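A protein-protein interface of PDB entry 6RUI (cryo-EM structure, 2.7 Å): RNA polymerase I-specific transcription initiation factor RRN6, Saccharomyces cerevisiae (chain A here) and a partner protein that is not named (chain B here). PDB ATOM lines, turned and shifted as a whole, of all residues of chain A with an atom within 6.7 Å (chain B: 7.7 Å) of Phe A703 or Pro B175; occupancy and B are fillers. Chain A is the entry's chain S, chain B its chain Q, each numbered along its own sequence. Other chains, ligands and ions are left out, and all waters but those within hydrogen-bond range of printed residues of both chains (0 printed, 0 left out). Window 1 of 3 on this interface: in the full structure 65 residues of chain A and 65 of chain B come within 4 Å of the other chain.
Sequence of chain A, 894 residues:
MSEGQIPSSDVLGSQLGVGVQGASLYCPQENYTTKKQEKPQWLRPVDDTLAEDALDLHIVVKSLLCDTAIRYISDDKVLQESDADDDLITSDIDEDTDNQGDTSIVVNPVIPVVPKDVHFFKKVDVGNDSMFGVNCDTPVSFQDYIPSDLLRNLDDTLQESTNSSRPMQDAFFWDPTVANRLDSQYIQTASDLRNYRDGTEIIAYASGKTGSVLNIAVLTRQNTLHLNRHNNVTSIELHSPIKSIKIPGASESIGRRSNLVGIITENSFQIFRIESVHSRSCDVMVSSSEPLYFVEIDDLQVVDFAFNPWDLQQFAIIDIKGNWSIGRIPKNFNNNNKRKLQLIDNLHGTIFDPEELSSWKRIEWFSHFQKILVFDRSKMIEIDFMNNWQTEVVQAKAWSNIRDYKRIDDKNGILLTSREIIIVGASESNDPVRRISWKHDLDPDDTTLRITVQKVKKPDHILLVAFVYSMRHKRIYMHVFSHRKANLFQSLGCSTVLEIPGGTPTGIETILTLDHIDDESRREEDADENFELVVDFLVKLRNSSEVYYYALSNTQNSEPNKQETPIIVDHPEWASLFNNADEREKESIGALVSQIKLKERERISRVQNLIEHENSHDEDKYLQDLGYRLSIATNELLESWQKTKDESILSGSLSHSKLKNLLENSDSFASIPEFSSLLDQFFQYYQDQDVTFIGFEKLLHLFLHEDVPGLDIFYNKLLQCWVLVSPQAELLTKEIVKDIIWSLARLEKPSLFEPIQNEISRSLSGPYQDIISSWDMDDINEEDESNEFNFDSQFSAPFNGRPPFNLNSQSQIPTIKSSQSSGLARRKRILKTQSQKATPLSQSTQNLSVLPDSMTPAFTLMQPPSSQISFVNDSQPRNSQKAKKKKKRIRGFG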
ATOM      1  N   LEU A 699     -15.434   0.464 -19.321  1.00  0.00           N
ATOM      2  CA  LEU A 699     -16.682   0.558 -18.586  1.00  0.00           C
ATOM      3  C   LEU A 699     -16.525   0.244 -17.104  1.00  0.00           C
ATOM      4  O   LEU A 699     -17.416   0.585 -16.322  1.00  0.00           O
ATOM      5  CB  LEU A 699     -17.722  -0.378 -19.226  1.00  0.00           C
ATOM      6  CG  LEU A 699     -19.215  -0.372 -18.920  1.00  0.00           C
ATOM      7  CD1 LEU A 699     -19.957  -0.709 -20.190  1.00  0.00           C
ATOM      8  CD2 LEU A 699     -19.550  -1.395 -17.863  1.00  0.00           C
ATOM      9  N   LEU A 700     -15.403  -0.330 -16.690  1.00  0.00           N
ATOM     10  CA  LEU A 700     -15.186  -0.792 -15.325  1.00  0.00           C
ATOM     11  C   LEU A 700     -14.881   0.348 -14.351  1.00  0.00           C
ATOM     12  O   LEU A 700     -14.778   0.115 -13.141  1.00  0.00           O
ATOM     13  CB  LEU A 700     -14.056  -1.829 -15.341  1.00  0.00           C
ATOM     14  CG  LEU A 700     -13.635  -2.731 -14.184  1.00  0.00           C
ATOM     15  CD1 LEU A 700     -14.797  -3.579 -13.719  1.00  0.00           C
ATOM     16  CD2 LEU A 700     -12.511  -3.611 -14.676  1.00  0.00           C
ATOM     17  N   HIS A 701     -14.792   1.580 -14.846  1.00  0.00           N
ATOM     18  CA  HIS A 701     -14.418   2.740 -14.048  1.00  0.00           C
ATOM     19  C   HIS A 701     -15.555   3.302 -13.206  1.00  0.00           C
ATOM     20  O   HIS A 701     -15.329   4.256 -12.456  1.00  0.00           O
ATOM     21  CB  HIS A 701     -13.900   3.835 -14.976  1.00  0.00           C
ATOM     22  CG  HIS A 701     -14.935   4.361 -15.920  1.00  0.00           C
ATOM     23  ND1 HIS A 701     -15.749   5.429 -15.612  1.00  0.00           N
ATOM     24  CD2 HIS A 701     -15.303   3.953 -17.157  1.00  0.00           C
ATOM     25  CE1 HIS A 701     -16.563   5.664 -16.624  1.00  0.00           C
ATOM     26  NE2 HIS A 701     -16.315   4.781 -17.572  1.00  0.00           N
ATOM     27  N   LEU A 702     -16.762   2.743 -13.312  1.00  0.00           N
ATOM     28  CA  LEU A 702     -17.935   3.357 -12.706  1.00  0.00           C
ATOM     29  C   LEU A 702     -17.961   3.230 -11.191  1.00  0.00           C
ATOM     30  O   LEU A 702     -18.744   3.926 -10.538  1.00  0.00           O
ATOM     31  CB  LEU A 702     -19.199   2.753 -13.305  1.00  0.00           C
ATOM     32  CG  LEU A 702     -19.351   3.116 -14.781  1.00  0.00           C
ATOM     33  CD1 LEU A 702     -20.535   2.410 -15.426  1.00  0.00           C
ATOM     34  CD2 LEU A 702     -19.485   4.619 -14.925  1.00  0.00           C
ATOM     35  N   PHE A 703     -17.095   2.372 -10.650  1.00  0.00           N
ATOM     36  CA  PHE A 703     -17.048   2.159  -9.182  1.00  0.00           C
ATOM     37  C   PHE A 703     -16.003   3.082  -8.540  1.00  0.00           C
ATOM     38  O   PHE A 703     -16.257   3.571  -7.428  1.00  0.00           O
ATOM     39  CB  PHE A 703     -16.813   0.678  -8.873  1.00  0.00           C
ATOM     40  CG  PHE A 703     -17.517  -0.286  -9.794  1.00  0.00           C
ATOM     41  CD1 PHE A 703     -18.675  -0.935  -9.395  1.00  0.00           C
ATOM     42  CD2 PHE A 703     -17.015  -0.561 -11.055  1.00  0.00           C
ATOM     43  CE1 PHE A 703     -19.315  -1.830 -10.236  1.00  0.00           C
ATOM     44  CE2 PHE A 703     -17.656  -1.456 -11.896  1.00  0.00           C
ATOM     45  CZ  PHE A 703     -18.806  -2.087 -11.486  1.00  0.00           C
ATOM     46  N   LEU A 704     -14.885   3.327  -9.232  1.00  0.00           N
ATOM     47  CA  LEU A 704     -13.799   4.153  -8.726  1.00  0.00           C
ATOM     48  C   LEU A 704     -13.965   5.620  -9.087  1.00  0.00           C
ATOM     49  O   LEU A 704     -13.301   6.467  -8.478  1.00  0.00           O
ATOM     50  CB  LEU A 704     -12.476   3.624  -9.266  1.00  0.00           C
ATOM     51  CG  LEU A 704     -12.232   2.177  -8.843  1.00  0.00           C
ATOM     52  CD1 LEU A 704     -11.001   1.619  -9.513  1.00  0.00           C
ATOM     53  CD2 LEU A 704     -12.114   2.089  -7.335  1.00  0.00           C
ATOM     54  N   HIS A 705     -14.826   5.912 -10.069  1.00  0.00           N
ATOM     55  CA  HIS A 705     -15.179   7.264 -10.518  1.00  0.00           C
ATOM     56  C   HIS A 705     -13.970   8.042 -11.019  1.00  0.00           C
ATOM     57  O   HIS A 705     -13.870   9.256 -10.833  1.00  0.00           O
ATOM     58  CB  HIS A 705     -15.920   8.038  -9.429  1.00  0.00           C
ATOM     59  CG  HIS A 705     -17.209   7.401  -9.036  1.00  0.00           C
ATOM     60  ND1 HIS A 705     -18.315   7.402  -9.856  1.00  0.00           N
ATOM     61  CD2 HIS A 705     -17.568   6.730  -7.919  1.00  0.00           C
ATOM     62  CE1 HIS A 705     -19.302   6.762  -9.259  1.00  0.00           C
ATOM     63  NE2 HIS A 705     -18.876   6.345  -8.081  1.00  0.00           N
ATOM     64  N   GLU A 706     -13.047   7.337 -11.663  1.00  0.00           N
ATOM     65  CA  GLU A 706     -11.910   7.971 -12.307  1.00  0.00           C
ATOM     66  C   GLU A 706     -11.673   7.341 -13.670  1.00  0.00           C
ATOM     67  O   GLU A 706     -12.535   6.628 -14.188  1.00  0.00           O
ATOM     68  CB  GLU A 706     -10.657   7.849 -11.447  1.00  0.00           C
ATOM     69  CG  GLU A 706     -10.256   6.424 -11.182  1.00  0.00           C
ATOM     70  CD  GLU A 706      -8.900   6.322 -10.541  1.00  0.00           C
ATOM     71  OE1 GLU A 706      -8.251   7.372 -10.353  1.00  0.00           O
ATOM     72  OE2 GLU A 706      -8.483   5.190 -10.229  1.00  0.00           O
ATOM     73  N   PHE A 714      -7.369  -2.263 -12.417  1.00  0.00           N
ATOM     74  CA  PHE A 714      -8.569  -2.181 -11.595  1.00  0.00           C
ATOM     75  C   PHE A 714      -8.415  -2.983 -10.321  1.00  0.00           C
ATOM     76  O   PHE A 714      -8.906  -2.569  -9.265  1.00  0.00           O
ATOM     77  CB  PHE A 714      -9.778  -2.678 -12.374  1.00  0.00           C
ATOM     78  CG  PHE A 714     -11.035  -2.706 -11.572  1.00  0.00           C
ATOM     79  CD1 PHE A 714     -11.683  -1.531 -11.246  1.00  0.00           C
ATOM     80  CD2 PHE A 714     -11.575  -3.908 -11.144  1.00  0.00           C
ATOM     81  CE1 PHE A 714     -12.847  -1.550 -10.496  1.00  0.00           C
ATOM     82  CE2 PHE A 714     -12.735  -3.937 -10.401  1.00  0.00           C
ATOM     83  CZ  PHE A 714     -13.373  -2.756 -10.074  1.00  0.00           C
ATOM     84  N   ILE A 740     -17.181  -9.565 -10.592  1.00  0.00           N
ATOM     85  CA  ILE A 740     -17.813  -8.452 -11.299  1.00  0.00           C
ATOM     86  C   ILE A 740     -17.835  -8.681 -12.803  1.00  0.00           C
ATOM     87  O   ILE A 740     -18.829  -8.359 -13.471  1.00  0.00           O
ATOM     88  CB  ILE A 740     -17.126  -7.130 -10.903  1.00  0.00           C
ATOM     89  CG1 ILE A 740     -17.426  -6.817  -9.436  1.00  0.00           C
ATOM     90  CG2 ILE A 740     -17.557  -5.958 -11.779  1.00  0.00           C
ATOM     91  CD1 ILE A 740     -18.915  -6.668  -9.134  1.00  0.00           C
ATOM     92  N   LEU A 744     -21.366  -8.692 -14.704  1.00  0.00           N
ATOM     93  CA  LEU A 744     -21.777  -8.231 -16.027  1.00  0.00           C
ATOM     94  C   LEU A 744     -21.513  -9.373 -17.005  1.00  0.00           C
ATOM     95  O   LEU A 744     -20.523  -9.414 -17.736  1.00  0.00           O
ATOM     96  CB  LEU A 744     -21.045  -6.948 -16.406  1.00  0.00           C
ATOM     97  CG  LEU A 744     -21.556  -6.110 -17.589  1.00  0.00           C
ATOM     98  CD1 LEU A 744     -21.338  -4.653 -17.298  1.00  0.00           C
ATOM     99  CD2 LEU A 744     -20.873  -6.430 -18.900  1.00  0.00           C
ATOM    100  N   PHE B 125     -20.573   5.138 -22.261  1.00  0.00           N
ATOM    101  CA  PHE B 125     -21.575   4.053 -22.432  1.00  0.00           C
ATOM    102  C   PHE B 125     -21.448   3.862 -23.942  1.00  0.00           C
ATOM    103  O   PHE B 125     -21.744   4.822 -24.674  1.00  0.00           O
ATOM    104  CB  PHE B 125     -23.002   4.553 -22.213  1.00  0.00           C
ATOM    105  CG  PHE B 125     -23.495   4.562 -20.791  1.00  0.00           C
ATOM    106  CD1 PHE B 125     -22.612   4.622 -19.728  1.00  0.00           C
ATOM    107  CD2 PHE B 125     -24.851   4.536 -20.520  1.00  0.00           C
ATOM    108  CE1 PHE B 125     -23.077   4.642 -18.425  1.00  0.00           C
ATOM    109  CE2 PHE B 125     -25.315   4.559 -19.217  1.00  0.00           C
ATOM    110  CZ  PHE B 125     -24.426   4.615 -18.172  1.00  0.00           C
ATOM    111  N   SER B 169     -30.438   0.633 -19.768  1.00  0.00           N
ATOM    112  CA  SER B 169     -29.239   0.385 -18.983  1.00  0.00           C
ATOM    113  C   SER B 169     -29.315  -0.953 -18.263  1.00  0.00           C
ATOM    114  O   SER B 169     -28.310  -1.666 -18.169  1.00  0.00           O
ATOM    115  CB  SER B 169     -29.014   1.509 -17.977  1.00  0.00           C
ATOM    116  OG  SER B 169     -29.939   1.431 -16.909  1.00  0.00           O
ATOM    117  N   LEU B 172     -28.390  -3.879 -20.557  1.00  0.00           N
ATOM    118  CA  LEU B 172     -26.954  -4.187 -20.824  1.00  0.00           C
ATOM    119  C   LEU B 172     -26.186  -4.689 -19.590  1.00  0.00           C
ATOM    120  O   LEU B 172     -24.962  -4.842 -19.705  1.00  0.00           O
ATOM    121  CB  LEU B 172     -26.285  -2.987 -21.500  1.00  0.00           C
ATOM    122  CG  LEU B 172     -26.339  -2.996 -23.028  1.00  0.00           C
ATOM    123  CD1 LEU B 172     -27.531  -3.796 -23.522  1.00  0.00           C
ATOM    124  CD2 LEU B 172     -26.383  -1.583 -23.586  1.00  0.00           C
ATOM    125  N   SER B 173     -26.872  -4.936 -18.470  1.00  0.00           N
ATOM    126  CA  SER B 173     -26.285  -5.500 -17.248  1.00  0.00           C
ATOM    127  C   SER B 173     -25.350  -4.509 -16.559  1.00  0.00           C
ATOM    128  O   SER B 173     -24.395  -4.900 -15.884  1.00  0.00           O
ATOM    129  CB  SER B 173     -25.570  -6.828 -17.530  1.00  0.00           C
ATOM    130  OG  SER B 173     -24.997  -7.372 -16.358  1.00  0.00           O
ATOM    131  N   LEU B 174     -25.650  -3.222 -16.700  1.00  0.00           N
ATOM    132  CA  LEU B 174     -24.710  -2.159 -16.398  1.00  0.00           C
ATOM    133  C   LEU B 174     -24.583  -1.922 -14.898  1.00  0.00           C
ATOM    134  O   LEU B 174     -25.551  -2.075 -14.153  1.00  0.00           O
ATOM    135  CB  LEU B 174     -25.142  -0.871 -17.076  1.00  0.00           C
ATOM    136  CG  LEU B 174     -25.004  -0.862 -18.590  1.00  0.00           C
ATOM    137  CD1 LEU B 174     -25.570   0.409 -19.181  1.00  0.00           C
ATOM    138  CD2 LEU B 174     -23.544  -1.020 -18.960  1.00  0.00           C
ATOM    139  N   PRO B 175     -23.390  -1.535 -14.438  1.00  0.00           N
ATOM    140  CA  PRO B 175     -23.225  -1.119 -13.040  1.00  0.00           C
ATOM    141  C   PRO B 175     -23.700   0.297 -12.742  1.00  0.00           C
ATOM    142  O   PRO B 175     -23.402   0.815 -11.661  1.00  0.00           O
ATOM    143  CB  PRO B 175     -21.710  -1.252 -12.826  1.00  0.00           C
ATOM    144  CG  PRO B 175     -21.125  -1.093 -14.162  1.00  0.00           C
ATOM    145  CD  PRO B 175     -22.098  -1.689 -15.123  1.00  0.00           C
ATOM    146  N   VAL B 176     -24.398   0.950 -13.671  1.00  0.00           N
ATOM    147  CA  VAL B 176     -25.143   2.153 -13.342  1.00  0.00           C
ATOM    148  C   VAL B 176     -26.430   1.739 -12.632  1.00  0.00           C
ATOM    149  O   VAL B 176     -26.934   0.622 -12.813  1.00  0.00           O
ATOM    150  CB  VAL B 176     -25.411   2.973 -14.622  1.00  0.00           C
ATOM    151  CG1 VAL B 176     -26.353   2.253 -15.554  1.00  0.00           C
ATOM    152  CG2 VAL B 176     -25.946   4.361 -14.324  1.00  0.00           C
ATOM    153  N   TYR B 177     -26.929   2.608 -11.756  1.00  0.00           N
ATOM    154  CA  TYR B 177     -28.175   2.376 -11.044  1.00  0.00           C
ATOM    155  C   TYR B 177     -28.993   3.654 -11.068  1.00  0.00           C
ATOM    156  O   TYR B 177     -28.572   4.665 -11.634  1.00  0.00           O
ATOM    157  CB  TYR B 177     -27.899   1.909  -9.616  1.00  0.00           C
ATOM    158  CG  TYR B 177     -27.144   0.621  -9.618  1.00  0.00           C
ATOM    159  CD1 TYR B 177     -27.782  -0.572  -9.919  1.00  0.00           C
ATOM    160  CD2 TYR B 177     -25.782   0.598  -9.366  1.00  0.00           C
ATOM    161  CE1 TYR B 177     -27.090  -1.754  -9.947  1.00  0.00           C
ATOM    162  CE2 TYR B 177     -25.083  -0.582  -9.386  1.00  0.00           C
ATOM    163  CZ  TYR B 177     -25.741  -1.750  -9.682  1.00  0.00           C
ATOM    164  OH  TYR B 177     -25.047  -2.927  -9.707  1.00  0.00           O
ATOM    165  N   THR B 178     -30.173   3.625 -10.440  1.00  0.00           N
ATOM    166  CA  THR B 178     -30.984   4.837 -10.383  1.00  0.00           C
ATOM    167  C   THR B 178     -30.422   5.860  -9.414  1.00  0.00           C
ATOM    168  O   THR B 178     -30.878   7.008  -9.417  1.00  0.00           O
ATOM    169  CB  THR B 178     -32.430   4.531  -9.993  1.00  0.00           C
ATOM    170  OG1 THR B 178     -33.205   5.726 -10.121  1.00  0.00           O
ATOM    171  CG2 THR B 178     -32.514   4.088  -8.568  1.00  0.00           C
ATOM    172  N   ASP B 180     -27.363   6.836  -9.759  1.00  0.00           N
ATOM    173  CA  ASP B 180     -26.600   7.677 -10.669  1.00  0.00           C
ATOM    174  C   ASP B 180     -27.506   8.510 -11.563  1.00  0.00           C
ATOM    175  O   ASP B 180     -27.190   9.665 -11.858  1.00  0.00           O
ATOM    176  CB  ASP B 180     -25.663   6.814 -11.497  1.00  0.00           C
ATOM    177  CG  ASP B 180     -24.517   6.278 -10.684  1.00  0.00           C
ATOM    178  OD1 ASP B 180     -24.132   6.941  -9.700  1.00  0.00           O
ATOM    179  OD2 ASP B 180     -23.994   5.201 -11.029  1.00  0.00           O
ATOM    180  N   TRP B 184     -26.974  12.376 -11.618  1.00  0.00           N
ATOM    181  CA  TRP B 184     -26.547  12.983 -12.913  1.00  0.00           C
ATOM    182  C   TRP B 184     -27.411  14.177 -13.334  1.00  0.00           C
ATOM    183  O   TRP B 184     -26.911  15.000 -14.109  1.00  0.00           O
ATOM    184  CB  TRP B 184     -26.510  11.931 -14.029  1.00  0.00           C
ATOM    185  CG  TRP B 184     -25.248  11.126 -14.068  1.00  0.00           C
ATOM    186  CD1 TRP B 184     -24.037  11.479 -13.552  1.00  0.00           C
ATOM    187  CD2 TRP B 184     -25.075   9.819 -14.642  1.00  0.00           C
ATOM    188  NE1 TRP B 184     -23.124  10.483 -13.764  1.00  0.00           N
ATOM    189  CE2 TRP B 184     -23.731   9.453 -14.431  1.00  0.00           C
ATOM    190  CE3 TRP B 184     -25.918   8.925 -15.308  1.00  0.00           C
ATOM    191  CZ2 TRP B 184     -23.215   8.234 -14.864  1.00  0.00           C
ATOM    192  CZ3 TRP B 184     -25.408   7.720 -15.733  1.00  0.00           C
ATOM    193  CH2 TRP B 184     -24.074   7.382 -15.516  1.00  0.00           C
ATOM    194  N   SER B 248     -27.733  -6.193 -11.764  1.00  0.00           N
ATOM    195  CA  SER B 248     -26.384  -6.572 -11.351  1.00  0.00           C
ATOM    196  C   SER B 248     -26.221  -6.181  -9.886  1.00  0.00           C
ATOM    197  O   SER B 248     -25.608  -5.171  -9.541  1.00  0.00           O
ATOM    198  CB  SER B 248     -25.338  -5.905 -12.231  1.00  0.00           C
ATOM    199  OG  SER B 248     -25.377  -4.501 -12.075  1.00  0.00           O
ATOM    200  N   GLN B 250     -24.555  -7.610  -7.579  1.00  0.00           N
ATOM    201  CA  GLN B 250     -23.169  -7.673  -7.140  1.00  0.00           C
ATOM    202  C   GLN B 250     -22.491  -6.320  -7.281  1.00  0.00           C
ATOM    203  O   GLN B 250     -21.691  -5.931  -6.425  1.00  0.00           O
ATOM    204  CB  GLN B 250     -22.417  -8.733  -7.939  1.00  0.00           C
ATOM    205  CG  GLN B 250     -22.875 -10.161  -7.694  1.00  0.00           C
ATOM    206  CD  GLN B 250     -24.047 -10.553  -8.563  1.00  0.00           C
ATOM    207  OE1 GLN B 250     -24.329  -9.903  -9.568  1.00  0.00           O
ATOM    208  NE2 GLN B 250     -24.745 -11.613  -8.175  1.00  0.00           N
ATOM    209  N   GLY B 251     -22.820  -5.577  -8.338  1.00  0.00           N
ATOM    210  CA  GLY B 251     -22.302  -4.229  -8.469  1.00  0.00           C
ATOM    211  C   GLY B 251     -22.925  -3.258  -7.487  1.00  0.00           C
ATOM    212  O   GLY B 251     -22.242  -2.368  -6.974  1.00  0.00           O
ATOM    213  N   LEU B 252     -24.219  -3.421  -7.204  1.00  0.00           N
ATOM    214  CA  LEU B 252     -24.914  -2.499  -6.311  1.00  0.00           C
ATOM    215  C   LEU B 252     -24.442  -2.647  -4.878  1.00  0.00           C
ATOM    216  O   LEU B 252     -24.331  -1.646  -4.164  1.00  0.00           O
ATOM    217  CB  LEU B 252     -26.423  -2.731  -6.378  1.00  0.00           C
ATOM    218  CG  LEU B 252     -27.369  -1.661  -5.829  1.00  0.00           C
ATOM    219  CD1 LEU B 252     -28.620  -1.757  -6.617  1.00  0.00           C
ATOM    220  CD2 LEU B 252     -27.721  -1.807  -4.364  1.00  0.00           C
ATOM    221  N   LEU B 254     -21.439  -3.869  -4.048  1.00  0.00           N
ATOM    222  CA  LEU B 254     -20.086  -3.334  -4.123  1.00  0.00           C
ATOM    223  C   LEU B 254     -20.086  -1.817  -4.158  1.00  0.00           C
ATOM    224  O   LEU B 254     -19.183  -1.185  -3.603  1.00  0.00           O
ATOM    225  CB  LEU B 254     -19.370  -3.887  -5.352  1.00  0.00           C
ATOM    226  CG  LEU B 254     -17.958  -3.381  -5.645  1.00  0.00           C
ATOM    227  CD1 LEU B 254     -17.020  -3.685  -4.487  1.00  0.00           C
ATOM    228  CD2 LEU B 254     -17.454  -3.980  -6.941  1.00  0.00           C
ATOM    229  N   LYS B 255     -21.101  -1.218  -4.780  1.00  0.00           N
ATOM    230  CA  LYS B 255     -21.274   0.223  -4.675  1.00  0.00           C
ATOM    231  C   LYS B 255     -21.568   0.618  -3.234  1.00  0.00           C
ATOM    232  O   LYS B 255     -20.877   1.467  -2.664  1.00  0.00           O
ATOM    233  CB  LYS B 255     -22.381   0.690  -5.618  1.00  0.00           C
ATOM    234  CG  LYS B 255     -22.464   2.195  -5.746  1.00  0.00           C
ATOM    235  CD  LYS B 255     -23.486   2.626  -6.786  1.00  0.00           C
ATOM    236  CE  LYS B 255     -23.577   4.148  -6.859  1.00  0.00           C
ATOM    237  NZ  LYS B 255     -24.610   4.622  -7.823  1.00  0.00           N
ATOM    238  N   MET B 258     -18.616   0.312  -1.091  1.00  0.00           N
ATOM    239  CA  MET B 258     -17.714   1.429  -1.316  1.00  0.00           C
ATOM    240  C   MET B 258     -18.283   2.767  -0.863  1.00  0.00           C
ATOM    241  O   MET B 258     -17.537   3.750  -0.841  1.00  0.00           O
ATOM    242  CB  MET B 258     -17.337   1.501  -2.790  1.00  0.00           C
ATOM    243  CG  MET B 258     -16.405   0.406  -3.245  1.00  0.00           C
ATOM    244  SD  MET B 258     -16.183   0.446  -5.024  1.00  0.00           S
ATOM    245  CE  MET B 258     -15.208   1.926  -5.190  1.00  0.00           C
ATOM    246  N   GLN B 259     -19.566   2.839  -0.498  1.00  0.00           N
ATOM    247  CA  GLN B 259     -20.098   4.088   0.037  1.00  0.00           C
ATOM    248  C   GLN B 259     -19.582   4.347   1.445  1.00  0.00           C
ATOM    249  O   GLN B 259     -19.051   5.427   1.730  1.00  0.00           O
ATOM    250  CB  GLN B 259     -21.627   4.073   0.023  1.00  0.00           C
ATOM    251  CG  GLN B 259     -22.228   4.078  -1.374  1.00  0.00           C
ATOM    252  CD  GLN B 259     -21.841   5.295  -2.187  1.00  0.00           C
ATOM    253  OE1 GLN B 259     -20.987   5.217  -3.065  1.00  0.00           O
ATOM    254  NE2 GLN B 259     -22.492   6.419  -1.922  1.00  0.00           N
ATOM    255  N   GLU B 346     -17.511  13.135  -5.857  1.00  0.00           N
ATOM    256  CA  GLU B 346     -18.782  12.449  -5.685  1.00  0.00           C
ATOM    257  C   GLU B 346     -19.534  12.889  -4.439  1.00  0.00           C
ATOM    258  O   GLU B 346     -20.766  12.881  -4.442  1.00  0.00           O
ATOM    259  CB  GLU B 346     -18.542  10.931  -5.642  1.00  0.00           C
ATOM    260  CG  GLU B 346     -19.775  10.045  -5.780  1.00  0.00           C
ATOM    261  CD  GLU B 346     -20.401   9.678  -4.448  1.00  0.00           C
ATOM    262  OE1 GLU B 346     -19.668   9.620  -3.438  1.00  0.00           O
ATOM    263  OE2 GLU B 346     -21.627   9.440  -4.414  1.00  0.00           O
ATOM    264  N   PHE B 438     -12.192   9.503  -5.592  1.00  0.00           N
ATOM    265  CA  PHE B 438     -12.907   8.536  -4.772  1.00  0.00           C
ATOM    266  C   PHE B 438     -12.059   7.318  -4.439  1.00  0.00           C
ATOM    267  O   PHE B 438     -12.433   6.526  -3.567  1.00  0.00           O
ATOM    268  CB  PHE B 438     -14.191   8.124  -5.491  1.00  0.00           C
ATOM    269  CG  PHE B 438     -15.144   7.355  -4.635  1.00  0.00           C
ATOM    270  CD1 PHE B 438     -15.855   7.994  -3.636  1.00  0.00           C
ATOM    271  CD2 PHE B 438     -15.331   5.998  -4.826  1.00  0.00           C
ATOM    272  CE1 PHE B 438     -16.731   7.297  -2.842  1.00  0.00           C
ATOM    273  CE2 PHE B 438     -16.206   5.294  -4.034  1.00  0.00           C
ATOM    274  CZ  PHE B 438     -16.911   5.946  -3.043  1.00  0.00           C
ATOM    275  N   ILE B 439     -10.922   7.148  -5.103  1.00  0.00           N
ATOM    276  CA  ILE B 439     -10.014   6.094  -4.687  1.00  0.00           C
ATOM    277  C   ILE B 439      -9.315   6.475  -3.388  1.00  0.00           C
ATOM    278  O   ILE B 439      -9.039   5.611  -2.550  1.00  0.00           O
ATOM    279  CB  ILE B 439      -9.027   5.797  -5.828  1.00  0.00           C
ATOM    280  CG1 ILE B 439      -8.296   7.079  -6.240  1.00  0.00           C
ATOM    281  CG2 ILE B 439      -9.776   5.231  -7.013  1.00  0.00           C
ATOM    282  CD1 ILE B 439      -7.172   6.902  -7.215  1.00  0.00           C
ATOM    283  N   LEU B 442     -11.185   6.830   0.484  1.00  0.00           N
ATOM    284  CA  LEU B 442     -11.282   5.516   1.101  1.00  0.00           C
ATOM    285  C   LEU B 442      -9.962   5.101   1.722  1.00  0.00           C
ATOM    286  O   LEU B 442      -9.951   4.430   2.753  1.00  0.00           O
ATOM    287  CB  LEU B 442     -11.719   4.492   0.061  1.00  0.00           C
ATOM    288  CG  LEU B 442     -13.095   4.756  -0.544  1.00  0.00           C
ATOM    289  CD1 LEU B 442     -13.385   3.786  -1.668  1.00  0.00           C
ATOM    290  CD2 LEU B 442     -14.144   4.650   0.541  1.00  0.00           C
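Among the printed residues, merely in contact across the chains: Phe A703 with Met B258 (3.0 Å), Phe A703 with Pro B175 (3.3 Å), Leu A744 with Ser B173 (3.3 Å), Glu A706 with Ile B439 (3.4 Å), Leu A704 with Phe B438 (3.5 Å), Phe A703 with Phe B438 (3.7 Å), Leu A699 with Pro B175 (3.8 Å), Leu A744 with Pro B175 (3.8 Å), Ile A740 with Leu B254 (3.8 Å), Leu A704 with Met B258 (3.8 Å), Leu A702 with Pro B175 (3.8 Å), Leu A699 with Leu B174 (3.8 Å), Leu A704 with Ile B439 (3.9 Å), His A705 with Phe B438 (3.9 Å) and Ile A740 with Gln B250 (3.9 Å).
Phe A703 touches just these residues of chain B: Pro B175, Met B258 and Phe B438.
Of the printed residues of chain A, Ile B439 touches Leu A704 (3.9 Å) and Glu A706 (3.4 Å).
Of the printed residues of chain A, Phe B438 touches Phe A703 (3.7 Å), Leu A704 (3.5 Å) and His A705 (3.9 Å).
Gly B251 touches none of the printed residues of chain A.
Asp B180 touches none of the printed residues of chain A.
The nearest residue of chain B that does not touch Phe A703 is Leu B254 (4.1 Å).
NE2 of His A705 sits close to O of Leu A702 (3.5 Å).
O of Ser B169 lies within hydrogen-bond range of N of Leu B174, at 3.4 Å.
The backbone carbonyl oxygen (O) of Leu B174 is in hydrogen-bond range of the side-chain hydroxyl (OG) of Ser B248 (3.2 Å).
Printed residues of chain A that touch a printed residue of chain B: Leu A699, Leu A702, Phe A703, Leu A704, His A705, Glu A706, Ile A740 and Leu A744.
Of the 23 printed residues of chain B, 8 touch a printed residue of chain A.
Hydrophobic or aromatic side chains of chain B that line the printed part of chain A: Leu B174, Pro B175, Leu B254, Met B258, Phe B438 and Ile B439.
Among the printed residues, no Asp or Glu carboxylate lies within 4 Å of a Lys or Arg side-chain nitrogen of the other chain.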
